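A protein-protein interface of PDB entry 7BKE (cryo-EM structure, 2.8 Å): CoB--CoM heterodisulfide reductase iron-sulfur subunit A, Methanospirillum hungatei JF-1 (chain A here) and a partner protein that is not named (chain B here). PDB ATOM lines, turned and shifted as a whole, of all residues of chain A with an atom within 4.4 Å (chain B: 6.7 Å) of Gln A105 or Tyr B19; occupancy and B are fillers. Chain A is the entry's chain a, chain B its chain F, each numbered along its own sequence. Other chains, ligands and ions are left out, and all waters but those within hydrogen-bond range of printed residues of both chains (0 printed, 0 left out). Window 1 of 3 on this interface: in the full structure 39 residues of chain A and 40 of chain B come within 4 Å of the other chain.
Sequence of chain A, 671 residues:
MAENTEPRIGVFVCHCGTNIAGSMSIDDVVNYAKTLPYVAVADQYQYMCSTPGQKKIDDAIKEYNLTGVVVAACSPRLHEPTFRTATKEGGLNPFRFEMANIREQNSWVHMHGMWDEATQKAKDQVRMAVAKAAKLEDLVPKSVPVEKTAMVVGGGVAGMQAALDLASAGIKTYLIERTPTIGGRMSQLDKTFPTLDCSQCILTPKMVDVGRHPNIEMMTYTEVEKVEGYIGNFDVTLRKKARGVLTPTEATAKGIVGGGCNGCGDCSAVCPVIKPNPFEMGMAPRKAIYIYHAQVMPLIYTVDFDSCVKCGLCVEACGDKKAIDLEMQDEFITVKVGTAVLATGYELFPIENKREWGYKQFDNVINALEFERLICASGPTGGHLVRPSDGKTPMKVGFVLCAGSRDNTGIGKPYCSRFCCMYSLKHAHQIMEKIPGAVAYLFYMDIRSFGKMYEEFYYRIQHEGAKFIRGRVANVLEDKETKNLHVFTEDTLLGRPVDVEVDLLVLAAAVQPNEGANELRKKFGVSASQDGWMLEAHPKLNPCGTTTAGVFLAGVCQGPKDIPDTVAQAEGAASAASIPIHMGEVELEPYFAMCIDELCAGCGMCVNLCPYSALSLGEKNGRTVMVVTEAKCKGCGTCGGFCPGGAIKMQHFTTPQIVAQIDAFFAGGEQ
Of the printed residues of chain A, Tyr B19 touches Ser A75 (3.7 Å), Pro A76 (3.3 Å), Arg A77 (3.5 Å), Asn A101 (3.2 Å) and Gln A105 (3.6 Å).
Printed residues of chain A within 4 Å of Ala B22: Glu A104 and Gln A105.
Printed residues of chain A within 4 Å of Asp B23: Ser A75, Arg A77, Asn A101, Glu A104 and Gln A105.
Printed residues of chain B within 4 Å of Glu A104: Ala B22, Asp B23 and Gly B26.
Of the printed residues of chain A, Ala B20 touches Arg A77.
Leu B24 touches none of the printed residues of chain A.
Trp B116 touches none of the printed residues of chain A.
The side-chain amide oxygen (OD1) of Asn A101 sits at hydrogen-bond distance from the backbone NH (N) of Arg A103.
The side-chain amide oxygen (OD1) of Asn A101 lies within hydrogen-bond range of the backbone NH (N) of Gln A105 (3.4 Å).
The guanidinium group (NH2) of Arg A103 is in salt-bridge range of the side-chain carboxylate (OE1) of Glu A104, at 3.3 Å.
O of Gln A105 lies within hydrogen-bond range of NZ of Lys A121, 3.2 Å away.
The side-chain amino group (NZ) of Lys A121 sits at hydrogen-bond distance from a ring nitrogen (NE2) of His A110, 3.0 Å away.
The backbone carbonyl oxygen (O) of Cys B14 lies within hydrogen-bond range of the backbone NH (N) of Tyr B19, at 2.9 Å.
Of the 12 printed residues of chain A, 9 touch a printed residue of chain B.
Printed residues of chain A that touch a printed residue of chain B: Ser A75, Pro A76, Arg A77, Asn A101, Glu A104, Gln A105, Val A109, His A110 and Lys A121.
Hydrophobic or aromatic side chains of chain A within 4 Å of the printed part of chain B: Pro A76, Val A109 and His A110.
Along chain A the printed residues that touch a printed residue of chain B span positions 75 to 121.
Of the 23 printed residues of chain B, 9 touch a printed residue of chain A.
Hydrophobic or aromatic side chains of chain B that line the printed part of chain A: Tyr B19, Ala B20, Ala B22 and Tyr B32.
Among the printed residues, no Asp or Glu carboxylate lies within 4 Å of a Lys or Arg side-chain nitrogen of the other chain.
The side-chain carboxylate of Asp B23 is in hydrogen-bond range of the side-chain hydroxyl of Ser A75 (2.8 Å).
The guanidinium group (NH1) of Arg A77 lies within hydrogen-bond range of the backbone carbonyl oxygen (O) of Asn B15 (3.0 Å).
The side-chain amide nitrogen of Asn A101 lies close to the side-chain hydroxyl of Tyr B19.
ND2 of Asn A101 sits at hydrogen-bond distance from OD2 of Asp B23, 3.5 Å away.
The side-chain amide nitrogen (NE2) of Gln A105 is in hydrogen-bond range of the side-chain carboxylate (OD2) of Asp B23 (3.2 Å).
The backbone NH (N) of Tyr B32 sits at hydrogen-bond distance from the backbone carbonyl oxygen (O) of Val A109 (3.4 Å).
A ring nitrogen (ND1) of His A110 lies within hydrogen-bond range of the backbone carbonyl oxygen of Tyr B32, 3.0 Å away.
O of Val B36 lies close to NZ of Lys A121, 3.3 Å away.
OG of Ser A75 touches CE1 of Tyr B19, 3.7 Å away.
CD of Pro A76 touches OH of Tyr B19, at 3.3 Å.
Arg A77 touches Tyr B19.
Arg A77 touches Ala B20 (NH2 to CB, 3.9 Å).
O of Glu A104 touches O of Ala B22, at 3.9 Å.
Glu A104 touches Asp B23.
Tyr B19 touches Gln A105.
NE2 of Gln A105 touches CB of Ala B22, 3.3 Å away.
Gly B26 touches Val A109.
Lys A121 touches Arg B37.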
ATOM      1  N   SER A  75      22.045  -5.235  27.410  1.00  0.00           N
ATOM      2  CA  SER A  75      22.302  -4.102  26.540  1.00  0.00           C
ATOM      3  C   SER A  75      23.770  -3.674  26.572  1.00  0.00           C
ATOM      4  O   SER A  75      24.429  -3.752  27.619  1.00  0.00           O
ATOM      5  CB  SER A  75      21.421  -2.929  26.943  1.00  0.00           C
ATOM      6  OG  SER A  75      21.924  -1.714  26.428  1.00  0.00           O
ATOM      7  N   PRO A  76      24.302  -3.203  25.440  1.00  0.00           N
ATOM      8  CA  PRO A  76      25.628  -2.579  25.460  1.00  0.00           C
ATOM      9  C   PRO A  76      25.717  -1.398  26.397  1.00  0.00           C
ATOM     10  O   PRO A  76      26.726  -1.258  27.095  1.00  0.00           O
ATOM     11  CB  PRO A  76      25.827  -2.152  24.004  1.00  0.00           C
ATOM     12  CG  PRO A  76      24.891  -2.966  23.232  1.00  0.00           C
ATOM     13  CD  PRO A  76      23.721  -3.214  24.093  1.00  0.00           C
ATOM     14  N   ARG A  77      24.680  -0.563  26.455  1.00  0.00           N
ATOM     15  CA  ARG A  77      24.690   0.579  27.357  1.00  0.00           C
ATOM     16  C   ARG A  77      24.824   0.145  28.803  1.00  0.00           C
ATOM     17  O   ARG A  77      25.239   0.944  29.648  1.00  0.00           O
ATOM     18  CB  ARG A  77      23.420   1.406  27.185  1.00  0.00           C
ATOM     19  CG  ARG A  77      23.018   1.634  25.745  1.00  0.00           C
ATOM     20  CD  ARG A  77      21.576   2.093  25.650  1.00  0.00           C
ATOM     21  NE  ARG A  77      21.258   3.158  26.595  1.00  0.00           N
ATOM     22  CZ  ARG A  77      21.743   4.397  26.531  1.00  0.00           C
ATOM     23  NH1 ARG A  77      22.570   4.746  25.561  1.00  0.00           N
ATOM     24  NH2 ARG A  77      21.393   5.292  27.442  1.00  0.00           N
ATOM     25  N   ASN A 101      22.200  -7.751  21.867  1.00  0.00           N
ATOM     26  CA  ASN A 101      21.186  -7.521  22.893  1.00  0.00           C
ATOM     27  C   ASN A 101      20.013  -8.460  22.658  1.00  0.00           C
ATOM     28  O   ASN A 101      19.141  -8.188  21.836  1.00  0.00           O
ATOM     29  CB  ASN A 101      20.741  -6.064  22.864  1.00  0.00           C
ATOM     30  CG  ASN A 101      19.790  -5.721  23.971  1.00  0.00           C
ATOM     31  OD1 ASN A 101      19.151  -6.587  24.544  1.00  0.00           O
ATOM     32  ND2 ASN A 101      19.687  -4.442  24.278  1.00  0.00           N
ATOM     33  N   ARG A 103      18.178  -9.641  25.398  1.00  0.00           N
ATOM     34  CA  ARG A 103      17.332  -9.649  26.607  1.00  0.00           C
ATOM     35  C   ARG A 103      16.367  -8.491  26.541  1.00  0.00           C
ATOM     36  O   ARG A 103      15.186  -8.728  26.352  1.00  0.00           O
ATOM     37  CB  ARG A 103      18.147  -9.446  27.888  1.00  0.00           C
ATOM     38  CG  ARG A 103      17.348  -9.602  29.170  1.00  0.00           C
ATOM     39  CD  ARG A 103      18.242  -9.418  30.371  1.00  0.00           C
ATOM     40  NE  ARG A 103      18.715  -8.056  30.516  1.00  0.00           N
ATOM     41  CZ  ARG A 103      19.182  -7.538  31.640  1.00  0.00           C
ATOM     42  NH1 ARG A 103      19.227  -8.265  32.737  1.00  0.00           N
ATOM     43  NH2 ARG A 103      19.576  -6.282  31.678  1.00  0.00           N
ATOM     44  N   GLU A 104      16.905  -7.291  26.630  1.00  0.00           N
ATOM     45  CA  GLU A 104      16.012  -6.150  26.723  1.00  0.00           C
ATOM     46  C   GLU A 104      15.296  -5.867  25.418  1.00  0.00           C
ATOM     47  O   GLU A 104      14.353  -5.075  25.406  1.00  0.00           O
ATOM     48  CB  GLU A 104      16.796  -4.923  27.175  1.00  0.00           C
ATOM     49  CG  GLU A 104      17.709  -5.235  28.339  1.00  0.00           C
ATOM     50  CD  GLU A 104      18.308  -4.010  28.963  1.00  0.00           C
ATOM     51  OE1 GLU A 104      19.527  -4.016  29.225  1.00  0.00           O
ATOM     52  OE2 GLU A 104      17.563  -3.037  29.192  1.00  0.00           O
ATOM     53  N   GLN A 105      15.718  -6.498  24.331  1.00  0.00           N
ATOM     54  CA  GLN A 105      15.084  -6.325  23.040  1.00  0.00           C
ATOM     55  C   GLN A 105      14.588  -7.625  22.446  1.00  0.00           C
ATOM     56  O   GLN A 105      14.079  -7.613  21.325  1.00  0.00           O
ATOM     57  CB  GLN A 105      16.048  -5.656  22.062  1.00  0.00           C
ATOM     58  CG  GLN A 105      16.610  -4.373  22.595  1.00  0.00           C
ATOM     59  CD  GLN A 105      16.965  -3.404  21.508  1.00  0.00           C
ATOM     60  OE1 GLN A 105      17.045  -3.772  20.341  1.00  0.00           O
ATOM     61  NE2 GLN A 105      17.192  -2.158  21.884  1.00  0.00           N
ATOM     62  N   ASN A 106      14.770  -8.751  23.125  1.00  0.00           N
ATOM     63  CA  ASN A 106      14.127  -9.988  22.711  1.00  0.00           C
ATOM     64  C   ASN A 106      13.255 -10.594  23.802  1.00  0.00           C
ATOM     65  O   ASN A 106      12.059 -10.787  23.586  1.00  0.00           O
ATOM     66  CB  ASN A 106      15.193 -10.976  22.242  1.00  0.00           C
ATOM     67  CG  ASN A 106      14.624 -12.087  21.432  1.00  0.00           C
ATOM     68  OD1 ASN A 106      13.530 -12.559  21.695  1.00  0.00           O
ATOM     69  ND2 ASN A 106      15.363 -12.521  20.435  1.00  0.00           N
ATOM     70  N   SER A 107      13.805 -10.866  24.986  1.00  0.00           N
ATOM     71  CA  SER A 107      13.080 -11.648  25.983  1.00  0.00           C
ATOM     72  C   SER A 107      11.971 -10.833  26.616  1.00  0.00           C
ATOM     73  O   SER A 107      10.794 -11.216  26.589  1.00  0.00           O
ATOM     74  CB  SER A 107      14.030 -12.127  27.072  1.00  0.00           C
ATOM     75  OG  SER A 107      14.937 -13.070  26.583  1.00  0.00           O
ATOM     76  N   VAL A 109      10.434  -8.381  25.790  1.00  0.00           N
ATOM     77  CA  VAL A 109       9.411  -7.887  24.883  1.00  0.00           C
ATOM     78  C   VAL A 109       8.718  -8.997  24.116  1.00  0.00           C
ATOM     79  O   VAL A 109       7.701  -8.730  23.466  1.00  0.00           O
ATOM     80  CB  VAL A 109       9.991  -6.852  23.903  1.00  0.00           C
ATOM     81  CG1 VAL A 109      10.483  -5.657  24.656  1.00  0.00           C
ATOM     82  CG2 VAL A 109      11.114  -7.462  23.117  1.00  0.00           C
ATOM     83  N   HIS A 110       9.231 -10.222  24.146  1.00  0.00           N
ATOM     84  CA  HIS A 110       8.556 -11.355  23.533  1.00  0.00           C
ATOM     85  C   HIS A 110       8.405 -12.488  24.526  1.00  0.00           C
ATOM     86  O   HIS A 110       8.593 -13.657  24.189  1.00  0.00           O
ATOM     87  CB  HIS A 110       9.291 -11.836  22.286  1.00  0.00           C
ATOM     88  CG  HIS A 110       9.733 -10.732  21.378  1.00  0.00           C
ATOM     89  ND1 HIS A 110       8.998  -9.586  21.188  1.00  0.00           N
ATOM     90  CD2 HIS A 110      10.838 -10.601  20.612  1.00  0.00           C
ATOM     91  CE1 HIS A 110       9.632  -8.793  20.346  1.00  0.00           C
ATOM     92  NE2 HIS A 110      10.753  -9.385  19.983  1.00  0.00           N
ATOM     93  N   LYS A 121      14.417 -14.550  16.313  1.00  0.00           N
ATOM     94  CA  LYS A 121      14.962 -13.207  16.471  1.00  0.00           C
ATOM     95  C   LYS A 121      16.341 -13.244  17.122  1.00  0.00           C
ATOM     96  O   LYS A 121      17.240 -12.492  16.732  1.00  0.00           O
ATOM     97  CB  LYS A 121      14.004 -12.341  17.281  1.00  0.00           C
ATOM     98  CG  LYS A 121      14.409 -10.890  17.333  1.00  0.00           C
ATOM     99  CD  LYS A 121      13.331 -10.038  17.938  1.00  0.00           C
ATOM    100  CE  LYS A 121      13.728  -8.597  17.910  1.00  0.00           C
ATOM    101  NZ  LYS A 121      12.664  -7.726  18.451  1.00  0.00           N
ATOM    102  N   ILE B  13      18.699   2.373  14.670  1.00  0.00           N
ATOM    103  CA  ILE B  13      18.304   3.243  15.764  1.00  0.00           C
ATOM    104  C   ILE B  13      19.549   3.853  16.385  1.00  0.00           C
ATOM    105  O   ILE B  13      20.569   3.178  16.539  1.00  0.00           O
ATOM    106  CB  ILE B  13      17.469   2.477  16.805  1.00  0.00           C
ATOM    107  CG1 ILE B  13      18.227   1.276  17.339  1.00  0.00           C
ATOM    108  CG2 ILE B  13      16.195   1.980  16.180  1.00  0.00           C
ATOM    109  CD1 ILE B  13      17.383   0.393  18.195  1.00  0.00           C
ATOM    110  N   CYS B  14      19.471   5.135  16.714  1.00  0.00           N
ATOM    111  CA  CYS B  14      20.596   5.798  17.340  1.00  0.00           C
ATOM    112  C   CYS B  14      20.793   5.273  18.752  1.00  0.00           C
ATOM    113  O   CYS B  14      19.911   4.661  19.348  1.00  0.00           O
ATOM    114  CB  CYS B  14      20.403   7.311  17.365  1.00  0.00           C
ATOM    115  SG  CYS B  14      19.308   7.928  18.614  1.00  0.00           S
ATOM    116  N   ASN B  15      21.986   5.506  19.279  1.00  0.00           N
ATOM    117  CA  ASN B  15      22.357   4.962  20.573  1.00  0.00           C
ATOM    118  C   ASN B  15      21.748   5.743  21.724  1.00  0.00           C
ATOM    119  O   ASN B  15      21.502   5.168  22.784  1.00  0.00           O
ATOM    120  CB  ASN B  15      23.876   4.956  20.693  1.00  0.00           C
ATOM    121  CG  ASN B  15      24.368   4.333  21.971  1.00  0.00           C
ATOM    122  OD1 ASN B  15      24.540   3.124  22.054  1.00  0.00           O
ATOM    123  ND2 ASN B  15      24.635   5.160  22.968  1.00  0.00           N
ATOM    124  N   TRP B  16      21.492   7.028  21.545  1.00  0.00           N
ATOM    125  CA  TRP B  16      21.252   7.900  22.676  1.00  0.00           C
ATOM    126  C   TRP B  16      19.786   8.184  22.949  1.00  0.00           C
ATOM    127  O   TRP B  16      19.463   8.629  24.052  1.00  0.00           O
ATOM    128  CB  TRP B  16      21.992   9.220  22.479  1.00  0.00           C
ATOM    129  CG  TRP B  16      23.450   9.009  22.433  1.00  0.00           C
ATOM    130  CD1 TRP B  16      24.208   8.822  21.326  1.00  0.00           C
ATOM    131  CD2 TRP B  16      24.336   8.919  23.547  1.00  0.00           C
ATOM    132  NE1 TRP B  16      25.514   8.634  21.673  1.00  0.00           N
ATOM    133  CE2 TRP B  16      25.622   8.690  23.035  1.00  0.00           C
ATOM    134  CE3 TRP B  16      24.170   9.015  24.928  1.00  0.00           C
ATOM    135  CZ2 TRP B  16      26.734   8.556  23.852  1.00  0.00           C
ATOM    136  CZ3 TRP B  16      25.273   8.880  25.736  1.00  0.00           C
ATOM    137  CH2 TRP B  16      26.538   8.655  25.198  1.00  0.00           C
ATOM    138  N   CYS B  17      18.896   7.972  21.989  1.00  0.00           N
ATOM    139  CA  CYS B  17      17.485   8.084  22.319  1.00  0.00           C
ATOM    140  C   CYS B  17      16.669   6.884  21.875  1.00  0.00           C
ATOM    141  O   CYS B  17      15.802   6.427  22.616  1.00  0.00           O
ATOM    142  CB  CYS B  17      16.894   9.354  21.726  1.00  0.00           C
ATOM    143  SG  CYS B  17      17.182  10.835  22.727  1.00  0.00           S
ATOM    144  N   SER B  18      16.933   6.338  20.698  1.00  0.00           N
ATOM    145  CA  SER B  18      16.087   5.242  20.251  1.00  0.00           C
ATOM    146  C   SER B  18      16.504   3.921  20.870  1.00  0.00           C
ATOM    147  O   SER B  18      15.648   3.106  21.221  1.00  0.00           O
ATOM    148  CB  SER B  18      16.095   5.150  18.738  1.00  0.00           C
ATOM    149  OG  SER B  18      15.419   6.257  18.188  1.00  0.00           O
ATOM    150  N   TYR B  19      17.806   3.686  21.018  1.00  0.00           N
ATOM    151  CA  TYR B  19      18.237   2.494  21.730  1.00  0.00           C
ATOM    152  C   TYR B  19      17.842   2.570  23.192  1.00  0.00           C
ATOM    153  O   TYR B  19      17.416   1.575  23.779  1.00  0.00           O
ATOM    154  CB  TYR B  19      19.738   2.307  21.594  1.00  0.00           C
ATOM    155  CG  TYR B  19      20.165   0.871  21.654  1.00  0.00           C
ATOM    156  CD1 TYR B  19      20.719   0.343  22.801  1.00  0.00           C
ATOM    157  CD2 TYR B  19      20.018   0.047  20.562  1.00  0.00           C
ATOM    158  CE1 TYR B  19      21.107  -0.964  22.856  1.00  0.00           C
ATOM    159  CE2 TYR B  19      20.399  -1.261  20.610  1.00  0.00           C
ATOM    160  CZ  TYR B  19      20.946  -1.761  21.759  1.00  0.00           C
ATOM    161  OH  TYR B  19      21.335  -3.074  21.807  1.00  0.00           O
ATOM    162  N   ALA B  20      17.959   3.755  23.789  1.00  0.00           N
ATOM    163  CA  ALA B  20      17.519   3.935  25.166  1.00  0.00           C
ATOM    164  C   ALA B  20      16.021   3.717  25.300  1.00  0.00           C
ATOM    165  O   ALA B  20      15.563   3.120  26.277  1.00  0.00           O
ATOM    166  CB  ALA B  20      17.901   5.327  25.654  1.00  0.00           C
ATOM    167  N   GLY B  21      15.238   4.195  24.333  1.00  0.00           N
ATOM    168  CA  GLY B  21      13.800   3.989  24.384  1.00  0.00           C
ATOM    169  C   GLY B  21      13.403   2.536  24.222  1.00  0.00           C
ATOM    170  O   GLY B  21      12.514   2.048  24.916  1.00  0.00           O
ATOM    171  N   ALA B  22      14.055   1.827  23.303  1.00  0.00           N
ATOM    172  CA  ALA B  22      13.794   0.401  23.152  1.00  0.00           C
ATOM    173  C   ALA B  22      14.180  -0.364  24.408  1.00  0.00           C
ATOM    174  O   ALA B  22      13.463  -1.278  24.837  1.00  0.00           O
ATOM    175  CB  ALA B  22      14.551  -0.138  21.943  1.00  0.00           C
ATOM    176  N   ASP B  23      15.312  -0.003  25.011  1.00  0.00           N
ATOM    177  CA  ASP B  23      15.730  -0.630  26.257  1.00  0.00           C
ATOM    178  C   ASP B  23      14.741  -0.352  27.375  1.00  0.00           C
ATOM    179  O   ASP B  23      14.448  -1.233  28.184  1.00  0.00           O
ATOM    180  CB  ASP B  23      17.119  -0.133  26.641  1.00  0.00           C
ATOM    181  CG  ASP B  23      18.212  -0.816  25.862  1.00  0.00           C
ATOM    182  OD1 ASP B  23      19.394  -0.617  26.197  1.00  0.00           O
ATOM    183  OD2 ASP B  23      17.887  -1.564  24.920  1.00  0.00           O
ATOM    184  N   LEU B  24      14.229   0.874  27.444  1.00  0.00           N
ATOM    185  CA  LEU B  24      13.242   1.213  28.458  1.00  0.00           C
ATOM    186  C   LEU B  24      11.946   0.439  28.251  1.00  0.00           C
ATOM    187  O   LEU B  24      11.322   0.001  29.220  1.00  0.00           O
ATOM    188  CB  LEU B  24      12.983   2.713  28.446  1.00  0.00           C
ATOM    189  CG  LEU B  24      11.935   3.207  29.432  1.00  0.00           C
ATOM    190  CD1 LEU B  24      12.220   2.663  30.812  1.00  0.00           C
ATOM    191  CD2 LEU B  24      11.917   4.715  29.453  1.00  0.00           C
ATOM    192  N   GLY B  26      11.714  -2.537  26.884  1.00  0.00           N
ATOM    193  CA  GLY B  26      12.022  -3.871  27.372  1.00  0.00           C
ATOM    194  C   GLY B  26      12.017  -3.955  28.885  1.00  0.00           C
ATOM    195  O   GLY B  26      11.454  -4.886  29.462  1.00  0.00           O
ATOM    196  N   TYR B  32       5.541  -6.522  22.140  1.00  0.00           N
ATOM    197  CA  TYR B  32       5.245  -6.199  20.755  1.00  0.00           C
ATOM    198  C   TYR B  32       5.733  -7.346  19.886  1.00  0.00           C
ATOM    199  O   TYR B  32       6.514  -8.182  20.348  1.00  0.00           O
ATOM    200  CB  TYR B  32       5.883  -4.863  20.340  1.00  0.00           C
ATOM    201  CG  TYR B  32       7.342  -4.677  20.643  1.00  0.00           C
ATOM    202  CD1 TYR B  32       8.309  -5.297  19.878  1.00  0.00           C
ATOM    203  CD2 TYR B  32       7.751  -3.826  21.652  1.00  0.00           C
ATOM    204  CE1 TYR B  32       9.636  -5.107  20.133  1.00  0.00           C
ATOM    205  CE2 TYR B  32       9.077  -3.633  21.914  1.00  0.00           C
ATOM    206  CZ  TYR B  32      10.016  -4.273  21.150  1.00  0.00           C
ATOM    207  OH  TYR B  32      11.348  -4.083  21.409  1.00  0.00           O
ATOM    208  N   VAL B  36      10.971  -6.846  13.936  1.00  0.00           N
ATOM    209  CA  VAL B  36      11.968  -5.833  13.620  1.00  0.00           C
ATOM    210  C   VAL B  36      13.290  -6.198  14.280  1.00  0.00           C
ATOM    211  O   VAL B  36      13.320  -6.579  15.452  1.00  0.00           O
ATOM    212  CB  VAL B  36      11.482  -4.444  14.076  1.00  0.00           C
ATOM    213  CG1 VAL B  36      12.506  -3.399  13.775  1.00  0.00           C
ATOM    214  CG2 VAL B  36      10.176  -4.106  13.396  1.00  0.00           C
ATOM    215  N   ARG B  37      14.381  -6.085  13.529  1.00  0.00           N
ATOM    216  CA  ARG B  37      15.728  -6.275  14.045  1.00  0.00           C
ATOM    217  C   ARG B  37      16.532  -5.003  13.830  1.00  0.00           C
ATOM    218  O   ARG B  37      16.481  -4.414  12.752  1.00  0.00           O
ATOM    219  CB  ARG B  37      16.426  -7.451  13.364  1.00  0.00           C
ATOM    220  CG  ARG B  37      15.897  -8.813  13.751  1.00  0.00           C
ATOM    221  CD  ARG B  37      14.838  -9.249  12.786  1.00  0.00           C
ATOM    222  NE  ARG B  37      14.635 -10.692  12.758  1.00  0.00           N
ATOM    223  CZ  ARG B  37      13.585 -11.307  13.283  1.00  0.00           C
ATOM    224  NH1 ARG B  37      12.645 -10.608  13.894  1.00  0.00           N
ATOM    225  NH2 ARG B  37      13.473 -12.621  13.195  1.00  0.00           N
ATOM    226  N   ALA B  38      17.291  -4.592  14.845  1.00  0.00           N
ATOM    227  CA  ALA B  38      17.923  -3.280  14.876  1.00  0.00           C
ATOM    228  C   ALA B  38      19.434  -3.370  14.696  1.00  0.00           C
ATOM    229  O   ALA B  38      20.042  -4.423  14.893  1.00  0.00           O
ATOM    230  CB  ALA B  38      17.604  -2.560  16.185  1.00  0.00           C
ATOM    231  N   ILE B  39      20.037  -2.239  14.330  1.00  0.00           N
ATOM    232  CA  ILE B  39      21.446  -2.174  13.970  1.00  0.00           C
ATOM    233  C   ILE B  39      22.262  -1.362  14.973  1.00  0.00           C
ATOM    234  O   ILE B  39      23.406  -1.715  15.261  1.00  0.00           O
ATOM    235  CB  ILE B  39      21.615  -1.612  12.541  1.00  0.00           C
ATOM    236  CG1 ILE B  39      21.189  -2.640  11.504  1.00  0.00           C
ATOM    237  CG2 ILE B  39      23.043  -1.211  12.271  1.00  0.00           C
ATOM    238  CD1 ILE B  39      22.247  -3.623  11.159  1.00  0.00           C
ATOM    239  N   ARG B  40      21.692  -0.298  15.540  1.00  0.00           N
ATOM    240  CA  ARG B  40      22.391   0.508  16.544  1.00  0.00           C
ATOM    241  C   ARG B  40      23.644   1.236  16.074  1.00  0.00           C
ATOM    242  O   ARG B  40      24.755   0.740  16.251  1.00  0.00           O
ATOM    243  CB  ARG B  40      22.768  -0.318  17.770  1.00  0.00           C
ATOM    244  CG  ARG B  40      23.185   0.563  18.924  1.00  0.00           C
ATOM    245  CD  ARG B  40      23.755  -0.220  20.066  1.00  0.00           C
ATOM    246  NE  ARG B  40      25.199  -0.366  19.972  1.00  0.00           N
ATOM    247  CZ  ARG B  40      26.065   0.342  20.680  1.00  0.00           C
ATOM    248  NH1 ARG B  40      25.636   1.253  21.538  1.00  0.00           N
ATOM    249  NH2 ARG B  40      27.359   0.136  20.530  1.00  0.00           N
ATOM    250  N   VAL B  41      23.476   2.374  15.413  1.00  0.00           N
ATOM    251  CA  VAL B  41      24.571   3.293  15.128  1.00  0.00           C
ATOM    252  C   VAL B  41      24.594   4.369  16.208  1.00  0.00           C
ATOM    253  O   VAL B  41      23.681   4.437  17.030  1.00  0.00           O
ATOM    254  CB  VAL B  41      24.417   3.901  13.732  1.00  0.00           C
ATOM    255  CG1 VAL B  41      24.590   2.834  12.691  1.00  0.00           C
ATOM    256  CG2 VAL B  41      23.055   4.546  13.596  1.00  0.00           C
ATOM    257  N   SER B  66      15.200   5.286  13.394  1.00  0.00           N
ATOM    258  CA  SER B  66      14.668   5.928  14.581  1.00  0.00           C
ATOM    259  C   SER B  66      15.757   6.751  15.244  1.00  0.00           C
ATOM    260  O   SER B  66      16.872   6.269  15.427  1.00  0.00           O
ATOM    261  CB  SER B  66      14.100   4.887  15.541  1.00  0.00           C
ATOM    262  OG  SER B  66      13.409   5.497  16.606  1.00  0.00           O
ATOM    263  N   VAL B 108      12.024   9.062  18.540  1.00  0.00           N
ATOM    264  CA  VAL B 108      11.691   8.440  19.813  1.00  0.00           C
ATOM    265  C   VAL B 108      12.687   8.929  20.849  1.00  0.00           C
ATOM    266  O   VAL B 108      13.899   8.797  20.658  1.00  0.00           O
ATOM    267  CB  VAL B 108      11.724   6.907  19.703  1.00  0.00           C
ATOM    268  CG1 VAL B 108      11.670   6.275  21.066  1.00  0.00           C
ATOM    269  CG2 VAL B 108      10.586   6.417  18.846  1.00  0.00           C
ATOM    270  N   TRP B 116       7.866   3.600  21.646  1.00  0.00           N
ATOM    271  CA  TRP B 116       8.633   2.625  20.877  1.00  0.00           C
ATOM    272  C   TRP B 116       7.816   1.371  20.604  1.00  0.00           C
ATOM    273  O   TRP B 116       7.846   0.829  19.494  1.00  0.00           O
ATOM    274  CB  TRP B 116       9.922   2.260  21.600  1.00  0.00           C
ATOM    275  CG  TRP B 116      10.640   1.157  20.924  1.00  0.00           C
ATOM    276  CD1 TRP B 116      10.648  -0.152  21.283  1.00  0.00           C
ATOM    277  CD2 TRP B 116      11.444   1.257  19.752  1.00  0.00           C
ATOM    278  NE1 TRP B 116      11.413  -0.878  20.410  1.00  0.00           N
ATOM    279  CE2 TRP B 116      11.913  -0.032  19.457  1.00  0.00           C
ATOM    280  CE3 TRP B 116      11.816   2.311  18.922  1.00  0.00           C
ATOM    281  CZ2 TRP B 116      12.733  -0.290  18.374  1.00  0.00           C
ATOM    282  CZ3 TRP B 116      12.624   2.050  17.848  1.00  0.00           C
ATOM    283  CH2 TRP B 116      13.075   0.763  17.582  1.00  0.00           C
